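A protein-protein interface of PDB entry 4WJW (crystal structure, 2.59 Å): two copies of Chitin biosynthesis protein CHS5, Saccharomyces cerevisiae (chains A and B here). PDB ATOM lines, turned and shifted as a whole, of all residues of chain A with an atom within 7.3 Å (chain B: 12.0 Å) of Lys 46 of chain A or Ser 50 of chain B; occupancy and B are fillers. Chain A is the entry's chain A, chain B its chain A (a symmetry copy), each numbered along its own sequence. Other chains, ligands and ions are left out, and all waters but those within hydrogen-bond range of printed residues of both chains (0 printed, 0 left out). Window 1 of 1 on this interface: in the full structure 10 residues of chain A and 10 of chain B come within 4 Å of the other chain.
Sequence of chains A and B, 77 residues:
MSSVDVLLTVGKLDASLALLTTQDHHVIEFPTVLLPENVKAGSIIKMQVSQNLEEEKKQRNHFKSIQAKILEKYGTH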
ATOM      1  N   VAL A   4     -19.737   7.666 -27.628  1.00  0.00           N
ATOM      2  CA  VAL A   4     -18.485   7.968 -26.942  1.00  0.00           C
ATOM      3  C   VAL A   4     -17.882   6.713 -26.319  1.00  0.00           C
ATOM      4  O   VAL A   4     -18.186   5.594 -26.733  1.00  0.00           O
ATOM      5  CB  VAL A   4     -18.707   9.034 -25.880  1.00  0.00           C
ATOM      6  N   ASP A   5     -17.025   6.906 -25.322  1.00  0.00           N
ATOM      7  CA  ASP A   5     -16.362   5.792 -24.650  1.00  0.00           C
ATOM      8  C   ASP A   5     -15.915   6.184 -23.246  1.00  0.00           C
ATOM      9  O   ASP A   5     -14.742   6.479 -23.019  1.00  0.00           O
ATOM     10  CB  ASP A   5     -15.174   5.310 -25.470  1.00  0.00           C
ATOM     11  N   VAL A   6     -16.854   6.183 -22.305  1.00  0.00           N
ATOM     12  CA  VAL A   6     -16.556   6.580 -20.935  1.00  0.00           C
ATOM     13  C   VAL A   6     -16.439   5.376 -20.006  1.00  0.00           C
ATOM     14  O   VAL A   6     -16.370   4.231 -20.453  1.00  0.00           O
ATOM     15  CB  VAL A   6     -17.622   7.537 -20.421  1.00  0.00           C
ATOM     16  N   LEU A   7     -16.410   5.657 -18.709  1.00  0.00           N
ATOM     17  CA  LEU A   7     -16.383   4.632 -17.674  1.00  0.00           C
ATOM     18  C   LEU A   7     -16.820   5.263 -16.358  1.00  0.00           C
ATOM     19  O   LEU A   7     -16.017   5.882 -15.660  1.00  0.00           O
ATOM     20  CB  LEU A   7     -14.998   4.019 -17.550  1.00  0.00           C
ATOM     21  N   LEU A   8     -18.097   5.110 -16.029  1.00  0.00           N
ATOM     22  CA  LEU A   8     -18.686   5.826 -14.903  1.00  0.00           C
ATOM     23  C   LEU A   8     -18.832   4.955 -13.658  1.00  0.00           C
ATOM     24  O   LEU A   8     -19.743   4.130 -13.569  1.00  0.00           O
ATOM     25  CB  LEU A   8     -20.038   6.397 -15.304  1.00  0.00           C
ATOM     26  N   THR A   9     -17.933   5.150 -12.698  1.00  0.00           N
ATOM     27  CA  THR A   9     -18.011   4.455 -11.418  1.00  0.00           C
ATOM     28  C   THR A   9     -19.232   4.932 -10.645  1.00  0.00           C
ATOM     29  O   THR A   9     -19.617   6.098 -10.735  1.00  0.00           O
ATOM     30  CB  THR A   9     -16.743   4.675 -10.607  1.00  0.00           C
ATOM     31  N   ILE A  44     -18.311  -0.366 -11.610  1.00  0.00           N
ATOM     32  CA  ILE A  44     -17.904   0.435 -12.757  1.00  0.00           C
ATOM     33  C   ILE A  44     -18.670   0.014 -14.005  1.00  0.00           C
ATOM     34  O   ILE A  44     -18.818  -1.172 -14.268  1.00  0.00           O
ATOM     35  CB  ILE A  44     -16.406   0.316 -12.984  1.00  0.00           C
ATOM     36  N   ILE A  45     -19.169   0.985 -14.762  1.00  0.00           N
ATOM     37  CA  ILE A  45     -19.862   0.687 -16.010  1.00  0.00           C
ATOM     38  C   ILE A  45     -18.971   1.023 -17.201  1.00  0.00           C
ATOM     39  O   ILE A  45     -17.799   1.359 -17.032  1.00  0.00           O
ATOM     40  CB  ILE A  45     -21.175   1.450 -16.091  1.00  0.00           C
ATOM     41  N   LYS A  46     -19.529   0.928 -18.403  1.00  0.00           N
ATOM     42  CA  LYS A  46     -18.793   1.257 -19.618  1.00  0.00           C
ATOM     43  C   LYS A  46     -19.731   1.839 -20.669  1.00  0.00           C
ATOM     44  O   LYS A  46     -20.043   1.187 -21.666  1.00  0.00           O
ATOM     45  CB  LYS A  46     -18.080   0.027 -20.161  1.00  0.00           C
ATOM     46  N   MET A  47     -20.172   3.072 -20.437  1.00  0.00           N
ATOM     47  CA  MET A  47     -21.145   3.723 -21.308  1.00  0.00           C
ATOM     48  C   MET A  47     -20.552   4.085 -22.666  1.00  0.00           C
ATOM     49  O   MET A  47     -19.349   3.951 -22.890  1.00  0.00           O
ATOM     50  CB  MET A  47     -21.703   4.967 -20.630  1.00  0.00           C
ATOM     51  N   GLN A  48     -21.412   4.545 -23.572  1.00  0.00           N
ATOM     52  CA  GLN A  48     -20.989   4.944 -24.909  1.00  0.00           C
ATOM     53  C   GLN A  48     -21.983   5.923 -25.528  1.00  0.00           C
ATOM     54  O   GLN A  48     -21.743   7.129 -25.567  1.00  0.00           O
ATOM     55  CB  GLN A  48     -20.821   3.723 -25.801  1.00  0.00           C
ATOM     56  N   SER A  50     -23.343   1.833 -26.865  1.00  0.00           N
ATOM     57  CA  SER A  50     -24.510   2.709 -26.838  1.00  0.00           C
ATOM     58  C   SER A  50     -24.587   3.587 -28.085  1.00  0.00           C
ATOM     59  O   SER A  50     -23.586   4.164 -28.502  1.00  0.00           O
ATOM     60  CB  SER A  50     -24.489   3.585 -25.582  1.00  0.00           C
ATOM     61  OG  SER A  50     -25.777   4.101 -25.296  1.00  0.00           O
ATOM     62  N   VAL B   4     -23.995  -7.765 -22.144  1.00  0.00           N
ATOM     63  CA  VAL B   4     -24.337  -8.505 -23.354  1.00  0.00           C
ATOM     64  C   VAL B   4     -23.856  -7.771 -24.602  1.00  0.00           C
ATOM     65  O   VAL B   4     -22.947  -6.943 -24.536  1.00  0.00           O
ATOM     66  CB  VAL B   4     -25.838  -8.743 -23.423  1.00  0.00           C
ATOM     67  N   ASP B   5     -24.470  -8.081 -25.740  1.00  0.00           N
ATOM     68  CA  ASP B   5     -24.096  -7.466 -27.009  1.00  0.00           C
ATOM     69  C   ASP B   5     -25.247  -7.520 -28.007  1.00  0.00           C
ATOM     70  O   ASP B   5     -25.269  -8.368 -28.898  1.00  0.00           O
ATOM     71  CB  ASP B   5     -22.863  -8.149 -27.584  1.00  0.00           C
ATOM     72  N   VAL B   6     -26.202  -6.608 -27.856  1.00  0.00           N
ATOM     73  CA  VAL B   6     -27.373  -6.585 -28.723  1.00  0.00           C
ATOM     74  C   VAL B   6     -27.285  -5.480 -29.770  1.00  0.00           C
ATOM     75  O   VAL B   6     -26.232  -4.874 -29.970  1.00  0.00           O
ATOM     76  CB  VAL B   6     -28.639  -6.421 -27.893  1.00  0.00           C
ATOM     77  N   LEU B   7     -28.407  -5.236 -30.438  1.00  0.00           N
ATOM     78  CA  LEU B   7     -28.532  -4.164 -31.417  1.00  0.00           C
ATOM     79  C   LEU B   7     -30.011  -3.873 -31.628  1.00  0.00           C
ATOM     80  O   LEU B   7     -30.683  -4.556 -32.402  1.00  0.00           O
ATOM     81  CB  LEU B   7     -27.859  -4.540 -32.727  1.00  0.00           C
ATOM     82  N   LEU B   8     -30.517  -2.862 -30.930  1.00  0.00           N
ATOM     83  CA  LEU B   8     -31.952  -2.605 -30.889  1.00  0.00           C
ATOM     84  C   LEU B   8     -32.375  -1.461 -31.806  1.00  0.00           C
ATOM     85  O   LEU B   8     -32.188  -0.288 -31.478  1.00  0.00           O
ATOM     86  CB  LEU B   8     -32.386  -2.319 -29.459  1.00  0.00           C
ATOM     87  N   PHE B  30     -37.680   1.156 -23.838  1.00  0.00           N
ATOM     88  CA  PHE B  30     -36.785   1.884 -22.944  1.00  0.00           C
ATOM     89  C   PHE B  30     -36.895   3.397 -23.092  1.00  0.00           C
ATOM     90  O   PHE B  30     -37.020   3.913 -24.203  1.00  0.00           O
ATOM     91  CB  PHE B  30     -35.345   1.445 -23.179  1.00  0.00           C
ATOM     92  N   ILE B  45     -29.214   1.151 -32.330  1.00  0.00           N
ATOM     93  CA  ILE B  45     -28.303   1.345 -31.207  1.00  0.00           C
ATOM     94  C   ILE B  45     -27.384   0.138 -31.060  1.00  0.00           C
ATOM     95  O   ILE B  45     -27.388  -0.760 -31.901  1.00  0.00           O
ATOM     96  CB  ILE B  45     -29.080   1.586 -29.922  1.00  0.00           C
ATOM     97  N   LYS B  46     -26.595   0.122 -29.991  1.00  0.00           N
ATOM     98  CA  LYS B  46     -25.695  -0.993 -29.719  1.00  0.00           C
ATOM     99  C   LYS B  46     -25.541  -1.199 -28.216  1.00  0.00           C
ATOM    100  O   LYS B  46     -24.492  -0.901 -27.643  1.00  0.00           O
ATOM    101  CB  LYS B  46     -24.340  -0.758 -30.368  1.00  0.00           C
ATOM    102  N   MET B  47     -26.593  -1.713 -27.587  1.00  0.00           N
ATOM    103  CA  MET B  47     -26.624  -1.883 -26.138  1.00  0.00           C
ATOM    104  C   MET B  47     -25.679  -2.984 -25.665  1.00  0.00           C
ATOM    105  O   MET B  47     -25.096  -3.709 -26.472  1.00  0.00           O
ATOM    106  CB  MET B  47     -28.044  -2.175 -25.676  1.00  0.00           C
ATOM    107  N   GLN B  48     -25.534  -3.100 -24.348  1.00  0.00           N
ATOM    108  CA  GLN B  48     -24.676  -4.115 -23.749  1.00  0.00           C
ATOM    109  C   GLN B  48     -25.099  -4.412 -22.313  1.00  0.00           C
ATOM    110  O   GLN B  48     -25.745  -5.423 -22.040  1.00  0.00           O
ATOM    111  CB  GLN B  48     -23.220  -3.674 -23.793  1.00  0.00           C
ATOM    112  N   SER B  50     -21.978  -1.169 -21.992  1.00  0.00           N
ATOM    113  CA  SER B  50     -22.862  -1.059 -20.836  1.00  0.00           C
ATOM    114  C   SER B  50     -22.505  -2.072 -19.751  1.00  0.00           C
ATOM    115  O   SER B  50     -22.272  -3.241 -20.045  1.00  0.00           O
ATOM    116  CB  SER B  50     -24.321  -1.243 -21.263  1.00  0.00           C
ATOM    117  OG  SER B  50     -25.210  -0.713 -20.295  1.00  0.00           O
ATOM    118  N   GLN B  51     -22.463  -1.598 -18.505  1.00  0.00           N
ATOM    119  CA  GLN B  51     -22.230  -2.416 -17.307  1.00  0.00           C
ATOM    120  C   GLN B  51     -21.163  -3.506 -17.449  1.00  0.00           C
ATOM    121  O   GLN B  51     -21.467  -4.705 -17.426  1.00  0.00           O
ATOM    122  CB  GLN B  51     -23.545  -3.048 -16.843  1.00  0.00           C
ATOM    123  CG  GLN B  51     -24.779  -2.212 -17.148  1.00  0.00           C
ATOM    124  CD  GLN B  51     -25.936  -2.537 -16.228  1.00  0.00           C
ATOM    125  OE1 GLN B  51     -26.004  -3.625 -15.658  1.00  0.00           O
ATOM    126  NE2 GLN B  51     -26.848  -1.586 -16.071  1.00  0.00           N
ATOM    127  N   ASN B  52     -19.913  -3.068 -17.585  1.00  0.00           N
ATOM    128  CA  ASN B  52     -18.748  -3.950 -17.536  1.00  0.00           C
ATOM    129  C   ASN B  52     -18.408  -4.192 -16.074  1.00  0.00           C
ATOM    130  O   ASN B  52     -17.970  -3.298 -15.371  1.00  0.00           O
ATOM    131  CB  ASN B  52     -17.571  -3.322 -18.326  1.00  0.00           C
ATOM    132  CG  ASN B  52     -16.238  -4.079 -18.178  1.00  0.00           C
ATOM    133  OD1 ASN B  52     -16.032  -4.839 -17.240  1.00  0.00           O
ATOM    134  ND2 ASN B  52     -15.347  -3.899 -19.163  1.00  0.00           N
ATOM    135  N   LEU B  53     -18.629  -5.410 -15.607  1.00  0.00           N
ATOM    136  CA  LEU B  53     -18.318  -5.721 -14.217  1.00  0.00           C
ATOM    137  C   LEU B  53     -17.083  -6.616 -14.143  1.00  0.00           C
ATOM    138  O   LEU B  53     -16.947  -7.446 -13.245  1.00  0.00           O
ATOM    139  CB  LEU B  53     -19.520  -6.370 -13.517  1.00  0.00           C
ATOM    140  CG  LEU B  53     -20.869  -5.633 -13.460  1.00  0.00           C
ATOM    141  CD1 LEU B  53     -21.544  -5.934 -12.131  1.00  0.00           C
ATOM    142  CD2 LEU B  53     -20.772  -4.119 -13.667  1.00  0.00           C
ATOM    143  N   GLU B  54     -16.194  -6.433 -15.114  1.00  0.00           N
ATOM    144  CA  GLU B  54     -14.870  -7.028 -15.078  1.00  0.00           C
ATOM    145  C   GLU B  54     -13.872  -6.011 -14.521  1.00  0.00           C
ATOM    146  O   GLU B  54     -12.970  -6.401 -13.789  1.00  0.00           O
ATOM    147  CB  GLU B  54     -14.445  -7.519 -16.473  1.00  0.00           C
ATOM    148  CG  GLU B  54     -13.105  -8.253 -16.519  1.00  0.00           C
ATOM    149  CD  GLU B  54     -11.911  -7.343 -16.710  1.00  0.00           C
ATOM    150  OE1 GLU B  54     -12.087  -6.223 -17.230  1.00  0.00           O
ATOM    151  OE2 GLU B  54     -10.793  -7.763 -16.344  1.00  0.00           O
ATOM    152  N   GLU B  55     -14.036  -4.724 -14.840  1.00  0.00           N
ATOM    153  CA  GLU B  55     -13.061  -3.735 -14.408  1.00  0.00           C
ATOM    154  C   GLU B  55     -13.285  -3.271 -12.968  1.00  0.00           C
ATOM    155  O   GLU B  55     -12.973  -2.123 -12.590  1.00  0.00           O
ATOM    156  CB  GLU B  55     -13.081  -2.545 -15.341  1.00  0.00           C
ATOM    157  CG  GLU B  55     -13.342  -2.900 -16.796  1.00  0.00           C
ATOM    158  CD  GLU B  55     -12.510  -2.058 -17.718  1.00  0.00           C
ATOM    159  OE1 GLU B  55     -11.390  -1.713 -17.280  1.00  0.00           O
ATOM    160  OE2 GLU B  55     -12.969  -1.754 -18.845  1.00  0.00           O
ATOM    161  N   GLU B  56     -13.879  -4.151 -12.174  1.00  0.00           N
ATOM    162  CA  GLU B  56     -14.086  -3.890 -10.755  1.00  0.00           C
ATOM    163  C   GLU B  56     -12.921  -4.408  -9.925  1.00  0.00           C
ATOM    164  O   GLU B  56     -12.726  -3.969  -8.792  1.00  0.00           O
ATOM    165  CB  GLU B  56     -15.400  -4.513 -10.280  1.00  0.00           C
ATOM    166  CG  GLU B  56     -16.585  -4.040 -11.092  1.00  0.00           C
ATOM    167  CD  GLU B  56     -17.930  -4.415 -10.493  1.00  0.00           C
ATOM    168  OE1 GLU B  56     -17.971  -4.979  -9.382  1.00  0.00           O
ATOM    169  OE2 GLU B  56     -18.959  -4.119 -11.132  1.00  0.00           O
ATOM    170  N   LYS B  58      -9.695  -4.268 -11.162  1.00  0.00           N
ATOM    171  CA  LYS B  58      -8.472  -3.480 -11.442  1.00  0.00           C
ATOM    172  C   LYS B  58      -8.250  -2.569 -10.249  1.00  0.00           C
ATOM    173  O   LYS B  58      -7.151  -2.454  -9.703  1.00  0.00           O
ATOM    174  CB  LYS B  58      -8.525  -2.600 -12.719  1.00  0.00           C
ATOM    175  CG  LYS B  58      -9.363  -3.021 -13.908  1.00  0.00           C
ATOM    176  CD  LYS B  58      -9.360  -4.462 -14.018  1.00  0.00           C
ATOM    177  CE  LYS B  58     -10.050  -5.021 -15.142  1.00  0.00           C
ATOM    178  NZ  LYS B  58      -9.904  -6.470 -14.712  1.00  0.00           N
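Printed residues of chain A that touch a printed residue of chain B: Ile 44, Lys 46 and Ser 50.
Of the 18 printed residues of chain B, 6 touch a printed residue of chain A.
Hydrophobic or aromatic side chains of chain B that line the printed part of chain A: Leu 53.
Among the printed residues, 7 pairs touch across the chains.
The side-chain amide oxygen of Asn 52 of chain B lies within hydrogen-bond range of the backbone NH of Glu 55 of chain B.
N of Glu 54 of chain B is in hydrogen-bond range of OD1 of Asn 52 of chain B, 2.7 Å away.
No residue of chain B comes within 4 Å of Asp 5 of chain A.
No residue of chain B comes within 4 Å of Val 6 of chain A.
No residue of chain B comes within 4 Å of Leu 7 of chain A.
No residue of chain B comes within 4 Å of Leu 8 of chain A.
Ile 44 of chain A touches just these residues of chain B: Asn 52 (2.5 Å), Leu 53 (3.6 Å) and Glu 56 (3.8 Å).
Printed residues of chain B within 4 Å of Lys 46 of chain A: Ser 50, Gln 51 and Asn 52.
Met 47 of chain A touches none of the printed residues of chain B.
No residue of chain B comes within 4 Å of Gln 48 of chain A.
Of the printed residues of chain B, Ser 50 of chain A touches Lys 46.
Leu 7 of chain B touches none of the printed residues of chain A.
Printed residues of chain A within 4 Å of Lys 46 of chain B: Ser 50.
Ser 50 of chain B touches just one residue of chain A: Lys 46.
Of the printed residues of chain A, Asn 52 of chain B touches Ile 44 (2.5 Å) and Lys 46 (3.9 Å).
Of the printed residues of chain A, Leu 53 of chain B touches Ile 44 (3.6 Å).
Printed residues of chain A within 4 Å of Glu 56 of chain B: Ile 44.
The nearest residue of chain B that does not touch Lys 46 of chain A is Glu 55 of chain B (5.6 Å).
The nearest residue of chain A that does not touch Ser 50 of chain B is Met 47 of chain A (4.9 Å).
The nearest printed residue of chain A that does not touch Lys 46 of chain B is Gln 48 of chain A (6.2 Å).
The backbone carbonyl oxygen (O) of Lys 46 of chain A is in hydrogen-bond range of the backbone NH (N) of Ser 50 of chain B (3.1 Å).
The backbone carbonyl oxygen (O) of Ile 44 of chain A lies close to the backbone carbonyl oxygen (O) of Asn 52 of chain B, 2.5 Å away.
The backbone carbonyl oxygen (O) of Lys 46 of chain B sits at hydrogen-bond distance from the backbone NH (N) of Ser 50 of chain A.
Among the printed residues, merely in contact across the chains: Ile 44 of chain A with Leu 53 of chain B, Ile 44 of chain A with Glu 56 of chain B, Lys 46 of chain A with Asn 52 of chain B and Lys 46 of chain A with Gln 51 of chain B.
Lys 46 of chain A touches Ser 50 of chain B, and with the chains exchanged Ser 50 of chain A touches Lys 46 of chain B.
Of the 7 pairs that touch across the chains among the printed residues, 2 have their exchanged pair printed and touching as well.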
